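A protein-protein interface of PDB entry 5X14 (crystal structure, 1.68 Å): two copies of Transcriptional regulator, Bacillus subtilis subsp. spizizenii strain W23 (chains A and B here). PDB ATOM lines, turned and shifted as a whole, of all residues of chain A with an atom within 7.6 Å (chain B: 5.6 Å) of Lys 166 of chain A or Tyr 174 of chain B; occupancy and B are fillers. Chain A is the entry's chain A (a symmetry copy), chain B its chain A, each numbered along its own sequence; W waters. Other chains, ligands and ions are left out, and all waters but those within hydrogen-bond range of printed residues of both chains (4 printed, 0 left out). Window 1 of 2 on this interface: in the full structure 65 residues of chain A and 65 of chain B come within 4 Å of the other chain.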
ATOM      1  N   ILE A  96      10.590  -2.588   7.836  1.00  0.00           N
ATOM      2  CA  ILE A  96       9.777  -1.474   8.259  1.00  0.00           C
ATOM      3  C   ILE A  96       8.672  -2.034   9.159  1.00  0.00           C
ATOM      4  O   ILE A  96       8.136  -3.132   8.955  1.00  0.00           O
ATOM      5  CB  ILE A  96       9.196  -0.572   7.135  1.00  0.00           C
ATOM      6  CG1 ILE A  96       8.456  -1.381   6.074  1.00  0.00           C
ATOM      7  CG2 ILE A  96      10.286   0.309   6.503  1.00  0.00           C
ATOM      8  CD1 ILE A  96       8.591  -0.780   4.673  1.00  0.00           C
ATOM      9  N   PRO A  97       8.368  -1.283  10.204  1.00  0.00           N
ATOM     10  CA  PRO A  97       7.421  -1.852  11.095  1.00  0.00           C
ATOM     11  C   PRO A  97       5.990  -1.706  10.628  1.00  0.00           C
ATOM     12  O   PRO A  97       5.694  -1.076   9.566  1.00  0.00           O
ATOM     13  CB  PRO A  97       7.674  -1.075  12.398  1.00  0.00           C
ATOM     14  CG  PRO A  97       8.151   0.150  12.000  1.00  0.00           C
ATOM     15  CD  PRO A  97       9.009  -0.098  10.778  1.00  0.00           C
ATOM     16  N   LEU A 137       4.663  23.331  13.420  1.00  0.00           N
ATOM     17  CA  LEU A 137       5.909  22.739  12.887  1.00  0.00           C
ATOM     18  C   LEU A 137       6.674  23.743  12.053  1.00  0.00           C
ATOM     19  O   LEU A 137       7.904  23.781  12.120  1.00  0.00           O
ATOM     20  CB  LEU A 137       5.603  21.505  12.053  1.00  0.00           C
ATOM     21  CG  LEU A 137       5.062  20.356  12.873  1.00  0.00           C
ATOM     22  CD1 LEU A 137       4.514  19.253  11.949  1.00  0.00           C
ATOM     23  CD2 LEU A 137       6.170  19.806  13.776  1.00  0.00           C
ATOM     24  N   HIS A 160      18.498  17.424  13.491  1.00  0.00           N
ATOM     25  CA  HIS A 160      17.303  18.165  13.861  1.00  0.00           C
ATOM     26  C   HIS A 160      16.499  18.573  12.618  1.00  0.00           C
ATOM     27  O   HIS A 160      15.281  18.447  12.567  1.00  0.00           O
ATOM     28  CB  HIS A 160      17.705  19.401  14.673  1.00  0.00           C
ATOM     29  CG  HIS A 160      16.591  20.029  15.429  1.00  0.00           C
ATOM     30  ND1 HIS A 160      16.816  21.022  16.357  1.00  0.00           N
ATOM     31  CD2 HIS A 160      15.255  19.792  15.430  1.00  0.00           C
ATOM     32  CE1 HIS A 160      15.650  21.381  16.882  1.00  0.00           C
ATOM     33  NE2 HIS A 160      14.694  20.642  16.356  1.00  0.00           N
ATOM     34  N   TYR A 161      17.207  19.062  11.614  1.00  0.00           N
ATOM     35  CA  TYR A 161      16.597  19.352  10.293  1.00  0.00           C
ATOM     36  C   TYR A 161      15.878  18.160   9.710  1.00  0.00           C
ATOM     37  O   TYR A 161      14.736  18.265   9.170  1.00  0.00           O
ATOM     38  CB  TYR A 161      17.701  19.845   9.385  1.00  0.00           C
ATOM     39  CG  TYR A 161      17.296  20.125   7.945  1.00  0.00           C
ATOM     40  CD1 TYR A 161      16.766  21.351   7.598  1.00  0.00           C
ATOM     41  CD2 TYR A 161      17.528  19.198   6.932  1.00  0.00           C
ATOM     42  CE1 TYR A 161      16.398  21.624   6.301  1.00  0.00           C
ATOM     43  CE2 TYR A 161      17.188  19.456   5.654  1.00  0.00           C
ATOM     44  CZ  TYR A 161      16.621  20.674   5.324  1.00  0.00           C
ATOM     45  OH  TYR A 161      16.289  20.945   4.021  1.00  0.00           O
ATOM     46  N   LEU A 162      16.504  16.977   9.822  1.00  0.00           N
ATOM     47  CA  LEU A 162      15.878  15.768   9.294  1.00  0.00           C
ATOM     48  C   LEU A 162      14.556  15.483   9.974  1.00  0.00           C
ATOM     49  O   LEU A 162      13.523  15.256   9.322  1.00  0.00           O
ATOM     50  CB  LEU A 162      16.817  14.554   9.395  1.00  0.00           C
ATOM     51  CG  LEU A 162      18.083  14.643   8.549  1.00  0.00           C
ATOM     52  CD1 LEU A 162      18.860  13.319   8.683  1.00  0.00           C
ATOM     53  CD2 LEU A 162      17.712  14.896   7.064  1.00  0.00           C
ATOM     54  N   VAL A 163      14.522  15.521  11.299  1.00  0.00           N
ATOM     55  CA  VAL A 163      13.247  15.215  11.990  1.00  0.00           C
ATOM     56  C   VAL A 163      12.162  16.279  11.713  1.00  0.00           C
ATOM     57  O   VAL A 163      11.006  15.923  11.566  1.00  0.00           O
ATOM     58  CB  VAL A 163      13.380  14.926  13.522  1.00  0.00           C
ATOM     59  CG1 VAL A 163      14.065  13.612  13.733  1.00  0.00           C
ATOM     60  CG2 VAL A 163      14.058  16.069  14.298  1.00  0.00           C
ATOM     61  N   LEU A 164      12.556  17.540  11.624  1.00  0.00           N
ATOM     62  CA  LEU A 164      11.598  18.604  11.436  1.00  0.00           C
ATOM     63  C   LEU A 164      11.068  18.584  10.036  1.00  0.00           C
ATOM     64  O   LEU A 164       9.853  18.711   9.836  1.00  0.00           O
ATOM     65  CB  LEU A 164      12.189  19.945  11.783  1.00  0.00           C
ATOM     66  CG  LEU A 164      11.861  20.437  13.167  1.00  0.00           C
ATOM     67  CD1 LEU A 164      12.716  21.654  13.482  1.00  0.00           C
ATOM     68  CD2 LEU A 164      10.346  20.749  13.129  1.00  0.00           C
ATOM     69  N   THR A 165      11.930  18.425   9.052  1.00  0.00           N
ATOM     70  CA  THR A 165      11.416  18.357   7.651  1.00  0.00           C
ATOM     71  C   THR A 165      10.555  17.123   7.420  1.00  0.00           C
ATOM     72  O   THR A 165       9.516  17.197   6.700  1.00  0.00           O
ATOM     73  CB  THR A 165      12.564  18.422   6.600  1.00  0.00           C
ATOM     74  OG1 THR A 165      13.474  17.316   6.771  1.00  0.00           O
ATOM     75  CG2 THR A 165      13.336  19.736   6.662  1.00  0.00           C
ATOM     76  N   LYS A 166      10.901  15.992   8.020  1.00  0.00           N
ATOM     77  CA  LYS A 166      10.053  14.820   7.925  1.00  0.00           C
ATOM     78  C   LYS A 166       8.637  15.105   8.466  1.00  0.00           C
ATOM     79  O   LYS A 166       7.636  14.793   7.837  1.00  0.00           O
ATOM     80  CB  LYS A 166      10.665  13.654   8.676  1.00  0.00           C
ATOM     81  CG  LYS A 166       9.882  12.375   8.613  1.00  0.00           C
ATOM     82  CD  LYS A 166       9.949  11.763   7.211  1.00  0.00           C
ATOM     83  CE  LYS A 166       9.362  10.412   7.136  1.00  0.00           C
ATOM     84  NZ  LYS A 166       7.894  10.498   6.933  1.00  0.00           N
ATOM     85  N   ALA A 167       8.582  15.763   9.614  1.00  0.00           N
ATOM     86  CA  ALA A 167       7.288  16.037  10.274  1.00  0.00           C
ATOM     87  C   ALA A 167       6.469  17.012   9.424  1.00  0.00           C
ATOM     88  O   ALA A 167       5.265  16.865   9.289  1.00  0.00           O
ATOM     89  CB  ALA A 167       7.513  16.603  11.678  1.00  0.00           C
ATOM     90  N   LEU A 168       7.142  18.008   8.859  1.00  0.00           N
ATOM     91  CA  LEU A 168       6.472  19.005   8.011  1.00  0.00           C
ATOM     92  C   LEU A 168       5.909  18.361   6.813  1.00  0.00           C
ATOM     93  O   LEU A 168       4.742  18.616   6.471  1.00  0.00           O
ATOM     94  CB  LEU A 168       7.448  20.066   7.542  1.00  0.00           C
ATOM     95  CG  LEU A 168       7.778  21.115   8.520  1.00  0.00           C
ATOM     96  CD1 LEU A 168       9.038  21.815   7.961  1.00  0.00           C
ATOM     97  CD2 LEU A 168       6.604  22.123   8.653  1.00  0.00           C
ATOM     98  N   GLU A 169       6.705  17.524   6.135  1.00  0.00           N
ATOM     99  CA  GLU A 169       6.252  16.810   4.920  1.00  0.00           C
ATOM    100  C   GLU A 169       5.069  15.916   5.267  1.00  0.00           C
ATOM    101  O   GLU A 169       4.083  15.827   4.517  1.00  0.00           O
ATOM    102  CB  GLU A 169       7.372  15.946   4.352  1.00  0.00           C
ATOM    103  CG  GLU A 169       8.340  16.742   3.512  1.00  0.00           C
ATOM    104  CD  GLU A 169       7.651  17.398   2.329  1.00  0.00           C
ATOM    105  OE1 GLU A 169       7.009  16.676   1.536  1.00  0.00           O
ATOM    106  OE2 GLU A 169       7.737  18.641   2.203  1.00  0.00           O
ATOM    107  N   ARG A 170       5.182  15.245   6.402  1.00  0.00           N
ATOM    108  CA  ARG A 170       4.113  14.306   6.895  1.00  0.00           C
ATOM    109  C   ARG A 170       2.762  15.015   7.052  1.00  0.00           C
ATOM    110  O   ARG A 170       1.684  14.568   6.541  1.00  0.00           O
ATOM    111  CB  ARG A 170       4.534  13.662   8.220  1.00  0.00           C
ATOM    112  CG  ARG A 170       3.580  12.592   8.758  1.00  0.00           C
ATOM    113  CD  ARG A 170       4.053  12.085  10.141  1.00  0.00           C
ATOM    114  NE  ARG A 170       3.794  13.165  11.075  1.00  0.00           N
ATOM    115  CZ  ARG A 170       4.582  13.590  12.038  1.00  0.00           C
ATOM    116  NH1 ARG A 170       5.726  12.996  12.300  1.00  0.00           N
ATOM    117  NH2 ARG A 170       4.195  14.650  12.739  1.00  0.00           N
ATOM    118  N   GLU A 171       2.799  16.138   7.738  1.00  0.00           N
ATOM    119  CA  GLU A 171       1.559  16.863   8.022  1.00  0.00           C
ATOM    120  C   GLU A 171       1.060  17.554   6.781  1.00  0.00           C
ATOM    121  O   GLU A 171      -0.155  17.598   6.550  1.00  0.00           O
ATOM    122  CB  GLU A 171       1.720  17.826   9.168  1.00  0.00           C
ATOM    123  CG  GLU A 171       2.050  17.161  10.490  1.00  0.00           C
ATOM    124  CD  GLU A 171       1.026  16.130  10.923  1.00  0.00           C
ATOM    125  OE1 GLU A 171      -0.214  16.322  10.626  1.00  0.00           O
ATOM    126  OE2 GLU A 171       1.470  15.125  11.495  1.00  0.00           O
ATOM    127  N   LYS A 172       1.971  18.120   5.976  1.00  0.00           N
ATOM    128  CA  LYS A 172       1.534  18.694   4.674  1.00  0.00           C
ATOM    129  C   LYS A 172       0.813  17.663   3.844  1.00  0.00           C
ATOM    130  O   LYS A 172      -0.224  17.928   3.226  1.00  0.00           O
ATOM    131  CB  LYS A 172       2.728  19.205   3.880  1.00  0.00           C
ATOM    132  CG  LYS A 172       3.311  20.474   4.386  1.00  0.00           C
ATOM    133  CD  LYS A 172       4.593  20.818   3.665  1.00  0.00           C
ATOM    134  CE  LYS A 172       5.098  22.184   4.102  1.00  0.00           C
ATOM    135  NZ  LYS A 172       6.447  22.516   3.504  1.00  0.00           N
ATOM    136  N   ASN A 173       1.373  16.463   3.781  1.00  0.00           N
ATOM    137  CA  ASN A 173       0.752  15.386   3.023  1.00  0.00           C
ATOM    138  C   ASN A 173      -0.627  14.977   3.600  1.00  0.00           C
ATOM    139  O   ASN A 173      -1.602  14.740   2.819  1.00  0.00           O
ATOM    140  CB  ASN A 173       1.663  14.149   2.971  1.00  0.00           C
ATOM    141  CG  ASN A 173       1.071  13.007   2.116  1.00  0.00           C
ATOM    142  OD1 ASN A 173       0.620  11.974   2.632  1.00  0.00           O
ATOM    143  ND2 ASN A 173       1.066  13.213   0.816  1.00  0.00           N
ATOM    144  N   ASP B 102       8.871   6.495  15.311  1.00  0.00           N
ATOM    145  CA  ASP B 102       9.416   5.949  14.065  1.00  0.00           C
ATOM    146  C   ASP B 102      10.897   5.826  14.385  1.00  0.00           C
ATOM    147  O   ASP B 102      11.586   6.843  14.516  1.00  0.00           O
ATOM    148  CB  ASP B 102       9.149   6.902  12.925  1.00  0.00           C
ATOM    149  CG  ASP B 102       9.763   6.423  11.588  1.00  0.00           C
ATOM    150  OD1 ASP B 102      10.755   5.645  11.589  1.00  0.00           O
ATOM    151  OD2 ASP B 102       9.202   6.838  10.564  1.00  0.00           O
ATOM    152  N   PHE B 104      13.405   4.706  12.740  1.00  0.00           N
ATOM    153  CA  PHE B 104      14.315   5.177  11.698  1.00  0.00           C
ATOM    154  C   PHE B 104      14.575   6.681  11.890  1.00  0.00           C
ATOM    155  O   PHE B 104      15.657   7.167  11.679  1.00  0.00           O
ATOM    156  CB  PHE B 104      13.755   4.907  10.246  1.00  0.00           C
ATOM    157  CG  PHE B 104      14.643   5.478   9.173  1.00  0.00           C
ATOM    158  CD1 PHE B 104      15.812   4.835   8.795  1.00  0.00           C
ATOM    159  CD2 PHE B 104      14.379   6.725   8.619  1.00  0.00           C
ATOM    160  CE1 PHE B 104      16.683   5.390   7.863  1.00  0.00           C
ATOM    161  CE2 PHE B 104      15.282   7.272   7.710  1.00  0.00           C
ATOM    162  CZ  PHE B 104      16.389   6.605   7.342  1.00  0.00           C
ATOM    163  N   MET B 105      13.551   7.410  12.257  1.00  0.00           N
ATOM    164  CA  MET B 105      13.659   8.864  12.412  1.00  0.00           C
ATOM    165  C   MET B 105      14.492   9.206  13.659  1.00  0.00           C
ATOM    166  O   MET B 105      15.165  10.232  13.688  1.00  0.00           O
ATOM    167  CB  MET B 105      12.288   9.550  12.408  1.00  0.00           C
ATOM    168  CG  MET B 105      11.603   9.526  10.985  1.00  0.00           C
ATOM    169  SD  MET B 105      12.577  10.146   9.720  1.00  0.00           S
ATOM    170  CE  MET B 105      13.091  11.784  10.308  1.00  0.00           C
ATOM    171  N   GLN B 126      16.651   2.199   3.671  1.00  0.00           N
ATOM    172  CA  GLN B 126      15.308   2.583   4.025  1.00  0.00           C
ATOM    173  C   GLN B 126      14.510   2.910   2.747  1.00  0.00           C
ATOM    174  O   GLN B 126      13.381   2.530   2.625  1.00  0.00           O
ATOM    175  CB  GLN B 126      15.300   3.747   5.001  1.00  0.00           C
ATOM    176  CG  GLN B 126      13.924   4.080   5.596  1.00  0.00           C
ATOM    177  CD  GLN B 126      13.404   3.045   6.600  1.00  0.00           C
ATOM    178  OE1 GLN B 126      12.248   3.158   7.001  1.00  0.00           O
ATOM    179  NE2 GLN B 126      14.263   2.154   7.106  1.00  0.00           N
ATOM    180  N   ARG B 130      11.059   1.101   1.496  1.00  0.00           N
ATOM    181  CA  ARG B 130       9.821   1.899   1.379  1.00  0.00           C
ATOM    182  C   ARG B 130       9.290   1.830  -0.061  1.00  0.00           C
ATOM    183  O   ARG B 130       8.080   1.787  -0.257  1.00  0.00           O
ATOM    184  CB  ARG B 130      10.043   3.349   1.816  1.00  0.00           C
ATOM    185  CG  ARG B 130      10.389   3.493   3.314  1.00  0.00           C
ATOM    186  CD  ARG B 130       9.333   3.935   4.168  1.00  0.00           C
ATOM    187  NE  ARG B 130       9.689   3.810   5.575  1.00  0.00           N
ATOM    188  CZ  ARG B 130       8.759   3.554   6.467  1.00  0.00           C
ATOM    189  NH1 ARG B 130       7.504   3.465   6.037  1.00  0.00           N
ATOM    190  NH2 ARG B 130       9.043   3.420   7.753  1.00  0.00           N
ATOM    191  N   GLU B 169      -0.300   7.631  -0.257  1.00  0.00           N
ATOM    192  CA  GLU B 169       0.221   9.012  -0.150  1.00  0.00           C
ATOM    193  C   GLU B 169       1.318   9.061   0.906  1.00  0.00           C
ATOM    194  O   GLU B 169       2.361   9.711   0.726  1.00  0.00           O
ATOM    195  CB  GLU B 169      -0.889   9.979   0.249  1.00  0.00           C
ATOM    196  CG  GLU B 169      -1.733  10.399  -0.930  1.00  0.00           C
ATOM    197  CD  GLU B 169      -0.906  11.097  -1.994  1.00  0.00           C
ATOM    198  OE1 GLU B 169      -0.235  12.100  -1.667  1.00  0.00           O
ATOM    199  OE2 GLU B 169      -0.912  10.630  -3.156  1.00  0.00           O
ATOM    200  N   ARG B 170       1.066   8.381   2.013  1.00  0.00           N
ATOM    201  CA  ARG B 170       2.034   8.329   3.166  1.00  0.00           C
ATOM    202  C   ARG B 170       3.402   7.784   2.735  1.00  0.00           C
ATOM    203  O   ARG B 170       4.496   8.386   2.989  1.00  0.00           O
ATOM    204  CB  ARG B 170       1.462   7.485   4.309  1.00  0.00           C
ATOM    205  CG  ARG B 170       2.304   7.461   5.588  1.00  0.00           C
ATOM    206  CD  ARG B 170       1.681   6.505   6.633  1.00  0.00           C
ATOM    207  NE  ARG B 170       1.913   5.161   6.137  1.00  0.00           N
ATOM    208  CZ  ARG B 170       1.066   4.155   6.137  1.00  0.00           C
ATOM    209  NH1 ARG B 170      -0.126   4.265   6.679  1.00  0.00           N
ATOM    210  NH2 ARG B 170       1.446   3.019   5.562  1.00  0.00           N
ATOM    211  N   GLU B 171       3.365   6.655   2.059  1.00  0.00           N
ATOM    212  CA  GLU B 171       4.612   5.999   1.663  1.00  0.00           C
ATOM    213  C   GLU B 171       5.257   6.741   0.524  1.00  0.00           C
ATOM    214  O   GLU B 171       6.488   6.859   0.487  1.00  0.00           O
ATOM    215  CB  GLU B 171       4.401   4.545   1.330  1.00  0.00           C
ATOM    216  CG  GLU B 171       3.918   3.709   2.499  1.00  0.00           C
ATOM    217  CD  GLU B 171       4.841   3.755   3.701  1.00  0.00           C
ATOM    218  OE1 GLU B 171       6.112   3.859   3.506  1.00  0.00           O
ATOM    219  OE2 GLU B 171       4.294   3.746   4.812  1.00  0.00           O
ATOM    220  N   LYS B 172       4.454   7.235  -0.430  1.00  0.00           N
ATOM    221  CA  LYS B 172       5.037   8.090  -1.500  1.00  0.00           C
ATOM    222  C   LYS B 172       5.773   9.266  -0.910  1.00  0.00           C
ATOM    223  O   LYS B 172       6.873   9.631  -1.337  1.00  0.00           O
ATOM    224  CB  LYS B 172       3.948   8.615  -2.426  1.00  0.00           C
ATOM    225  CG  LYS B 172       3.392   7.607  -3.362  1.00  0.00           C
ATOM    226  CD  LYS B 172       2.201   8.150  -4.115  1.00  0.00           C
ATOM    227  CE  LYS B 172       1.733   7.152  -5.162  1.00  0.00           C
ATOM    228  NZ  LYS B 172       0.463   7.597  -5.854  1.00  0.00           N
ATOM    229  N   ASN B 173       5.156   9.915   0.068  1.00  0.00           N
ATOM    230  CA  ASN B 173       5.784  11.055   0.722  1.00  0.00           C
ATOM    231  C   ASN B 173       7.081  10.663   1.474  1.00  0.00           C
ATOM    232  O   ASN B 173       8.108  11.409   1.409  1.00  0.00           O
ATOM    233  CB  ASN B 173       4.816  11.730   1.707  1.00  0.00           C
ATOM    234  CG  ASN B 173       5.419  12.986   2.370  1.00  0.00           C
ATOM    235  OD1 ASN B 173       5.765  12.992   3.561  1.00  0.00           O
ATOM    236  ND2 ASN B 173       5.552  14.036   1.588  1.00  0.00           N
ATOM    237  N   TYR B 174       7.097   9.484   2.070  1.00  0.00           N
ATOM    238  CA  TYR B 174       8.304   8.995   2.760  1.00  0.00           C
ATOM    239  C   TYR B 174       9.451   8.763   1.771  1.00  0.00           C
ATOM    240  O   TYR B 174      10.627   9.135   2.005  1.00  0.00           O
ATOM    241  CB  TYR B 174       7.958   7.738   3.545  1.00  0.00           C
ATOM    242  CG  TYR B 174       8.719   7.527   4.837  1.00  0.00           C
ATOM    243  CD1 TYR B 174      10.110   7.558   4.870  1.00  0.00           C
ATOM    244  CD2 TYR B 174       8.057   7.157   5.997  1.00  0.00           C
ATOM    245  CE1 TYR B 174      10.784   7.335   6.031  1.00  0.00           C
ATOM    246  CE2 TYR B 174       8.769   6.917   7.195  1.00  0.00           C
ATOM    247  CZ  TYR B 174      10.122   6.982   7.194  1.00  0.00           C
ATOM    248  OH  TYR B 174      10.764   6.717   8.392  1.00  0.00           O
ATOM    249  N   VAL B 175       9.106   8.167   0.628  1.00  0.00           N
ATOM    250  CA  VAL B 175      10.037   7.897  -0.431  1.00  0.00           C
ATOM    251  C   VAL B 175      10.613   9.200  -0.933  1.00  0.00           C
ATOM    252  O   VAL B 175      11.860   9.322  -1.105  1.00  0.00           O
ATOM    253  CB  VAL B 175       9.369   7.054  -1.571  1.00  0.00           C
ATOM    254  CG1 VAL B 175      10.169   7.146  -2.893  1.00  0.00           C
ATOM    255  CG2 VAL B 175       9.208   5.607  -1.051  1.00  0.00           C
ATOM    256  N   SER B 176       9.735  10.173  -1.243  1.00  0.00           N
ATOM    257  CA  SER B 176      10.181  11.475  -1.749  1.00  0.00           C
ATOM    258  C   SER B 176      11.114  12.181  -0.781  1.00  0.00           C
ATOM    259  O   SER B 176      12.151  12.739  -1.183  1.00  0.00           O
ATOM    260  CB  SER B 176       8.974  12.353  -2.010  1.00  0.00           C
ATOM    261  OG  SER B 176       8.347  11.897  -3.178  1.00  0.00           O
ATOM    262  N   TRP B 177      10.762  12.166   0.487  1.00  0.00           N
ATOM    263  CA  TRP B 177      11.628  12.709   1.538  1.00  0.00           C
ATOM    264  C   TRP B 177      12.994  12.015   1.617  1.00  0.00           C
ATOM    265  O   TRP B 177      14.051  12.666   1.578  1.00  0.00           O
ATOM    266  CB  TRP B 177      10.912  12.687   2.882  1.00  0.00           C
ATOM    267  CG  TRP B 177      11.734  13.252   3.996  1.00  0.00           C
ATOM    268  CD1 TRP B 177      11.872  14.583   4.347  1.00  0.00           C
ATOM    269  CD2 TRP B 177      12.559  12.528   4.896  1.00  0.00           C
ATOM    270  NE1 TRP B 177      12.754  14.705   5.367  1.00  0.00           N
ATOM    271  CE2 TRP B 177      13.153  13.461   5.760  1.00  0.00           C
ATOM    272  CE3 TRP B 177      12.828  11.156   5.077  1.00  0.00           C
ATOM    273  CZ2 TRP B 177      14.023  13.087   6.780  1.00  0.00           C
ATOM    274  CZ3 TRP B 177      13.673  10.777   6.093  1.00  0.00           C
ATOM    275  CH2 TRP B 177      14.266  11.731   6.926  1.00  0.00           C
ATOM    276  N   LEU B 178      12.988  10.685   1.590  1.00  0.00           N
ATOM    277  CA  LEU B 178      14.262   9.974   1.587  1.00  0.00           C
ATOM    278  C   LEU B 178      15.173  10.320   0.376  1.00  0.00           C
ATOM    279  O   LEU B 178      16.363  10.428   0.514  1.00  0.00           O
ATOM    280  CB  LEU B 178      14.078   8.459   1.643  1.00  0.00           C
ATOM    281  CG  LEU B 178      13.493   7.913   2.948  1.00  0.00           C
ATOM    282  CD1 LEU B 178      12.892   6.505   2.758  1.00  0.00           C
ATOM    283  CD2 LEU B 178      14.557   7.896   4.055  1.00  0.00           C
ATOM    284  N   GLU B 179      14.566  10.473  -0.807  1.00  0.00           N
ATOM    285  CA  GLU B 179      15.295  10.822  -2.006  1.00  0.00           C
ATOM    286  C   GLU B 179      15.908  12.188  -1.816  1.00  0.00           C
ATOM    287  O   GLU B 179      17.071  12.422  -2.184  1.00  0.00           O
ATOM    288  CB  GLU B 179      14.289  10.803  -3.204  1.00  0.00           C
ATOM    289  CG  GLU B 179      13.881   9.400  -3.640  1.00  0.00           C
ATOM    290  CD  GLU B 179      12.796   9.370  -4.706  1.00  0.00           C
ATOM    291  OE1 GLU B 179      12.117  10.376  -4.928  1.00  0.00           O
ATOM    292  OE2 GLU B 179      12.622   8.294  -5.324  1.00  0.00           O
HETATM  293  O   HOH W   1       2.550  11.691  -1.348  1.00  0.00           O
HETATM  294  O   HOH W   2       4.189  16.737   1.793  1.00  0.00           O
HETATM  295  O   HOH W   3      -1.270  10.258   3.709  1.00  0.00           O
HETATM  296  O   HOH W   4       7.455  12.743   5.743  1.00  0.00           O
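The side-chain carboxylate (OE1) of Glu 169 of chain B sits at hydrogen-bond distance from the side-chain amide nitrogen (ND2) of Asn 173 of chain A (3.0 Å).
ND2 of Asn 173 of chain B sits at hydrogen-bond distance from OE1 of Glu 169 of chain A (3.0 Å).
The indole nitrogen (NE1) of Trp 177 of chain B sits at hydrogen-bond distance from the side-chain hydroxyl (OG1) of Thr 165 of chain A (3.1 Å).
N of Lys 166 of chain A sits close to NE1 of Trp 177 of chain B.
OD1 of Asp 102 of chain B is in hydrogen-bond range of N of Met 105 of chain B (3.4 Å).
NE of Arg 130 of chain B sits at hydrogen-bond distance from OE1 of Gln 126 of chain B (3.0 Å).
The side-chain carboxylate (OE1) of Glu 171 of chain B lies within salt-bridge range of the guanidinium group (NH1) of Arg 130 of chain B, at 2.9 Å.
The side-chain carboxylate (OE2) of Glu 171 of chain B lies within salt-bridge range of the guanidinium group (NH2) of Arg 170 of chain B.
OE2 of Glu 171 of chain A lies within salt-bridge range of NH2 of Arg 170 of chain A.
Gln 126 of chain B touches Ile 96 of chain A (OE1 to CG2, 3.5 Å).
Arg 130 of chain B touches Ile 96 of chain A.
O of Leu 162 of chain A touches CE of Met 105 of chain B, 3.6 Å away.
CZ2 of Trp 177 of chain B touches O of Leu 162 of chain A, 3.4 Å away.
Val 163 of chain A touches Met 105 of chain B.
Lys 166 of chain A touches Met 105 of chain B.
Lys 166 of chain A touches Tyr 174 of chain B (NZ to CD2, 3.5 Å).
OD1 of Asn 173 of chain B touches N of Arg 170 of chain A, 3.7 Å away.
OD1 of Asn 173 of chain A touches N of Arg 170 of chain B (3.7 Å).
Asn 173 of chain B touches Asn 173 of chain A.
Of the printed residues of chain B, Ile 96 of chain A touches Gln 126 (3.5 Å) and Arg 130 (3.6 Å).
Lys 166 of chain A touches just these residues of chain B: Met 105, Tyr 174 and Trp 177.
Leu 168 of chain A touches none of the printed residues of chain B.
Printed residues of chain A within 4 Å of Gln 126 of chain B: Ile 96.
Of the printed residues of chain A, Glu 169 of chain B touches Asn 173.
Of the printed residues of chain A, Asn 173 of chain B touches Glu 169, Arg 170 and Asn 173.
Of chain A, only Lys 166 (3.5 Å) comes within 4 Å of Tyr 174 of chain B.
Leu 178 of chain B touches none of the printed residues of chain A.
The nearest residue of chain B that does not touch Lys 166 of chain A is Asn 173 of chain B (4.7 Å).
The nearest printed residue of chain A that does not touch Tyr 174 of chain B is Ile 96 of chain A (6.7 Å).
The nearest printed residue of chain B that does not touch Arg 170 of chain A is Arg 170 of chain B (6.2 Å).
Of the 17 printed residues of chain A, 8 touch a printed residue of chain B.
Printed residues of chain B that touch a printed residue of chain A: Met 105, Gln 126, Arg 130, Glu 169, Arg 170, Asn 173, Tyr 174 and Trp 177.
Among the printed residues, 14 pairs touch across the chains.
Among the printed residues, no Asp or Glu carboxylate lies within 4 Å of a Lys or Arg side-chain nitrogen of the other chain.
Glu 169 of chain A touches Asn 173 of chain B, and with the chains exchanged Asn 173 of chain A touches Glu 169 of chain B.
Arg 170 of chain A touches Asn 173 of chain B, and with the chains exchanged Asn 173 of chain A touches Arg 170 of chain B.
Asn 173 of chain B touches its own counterpart, Asn 173 of chain A.
Of the 14 pairs that touch across the chains among the printed residues, 5 have their exchanged pair printed and touching as well.
Water W3 lies within hydrogen-bond range of OD1 of Asn 173 of chain A (2.8 Å) and N of Arg 170 of chain B (3.4 Å).
Water W1 lies within hydrogen-bond range of the side-chain carboxylate (OE1) of Glu 169 of chain B, the side-chain amide nitrogen (ND2) of Asn 173 of chain A and the backbone NH (N) of Asn 173 of chain B.
Water W2 lies within hydrogen-bond range of OE1 of Glu 169 of chain A (2.8 Å), ND2 of Asn 173 of chain B (3.0 Å) and N of Asn 173 of chain A (3.5 Å).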
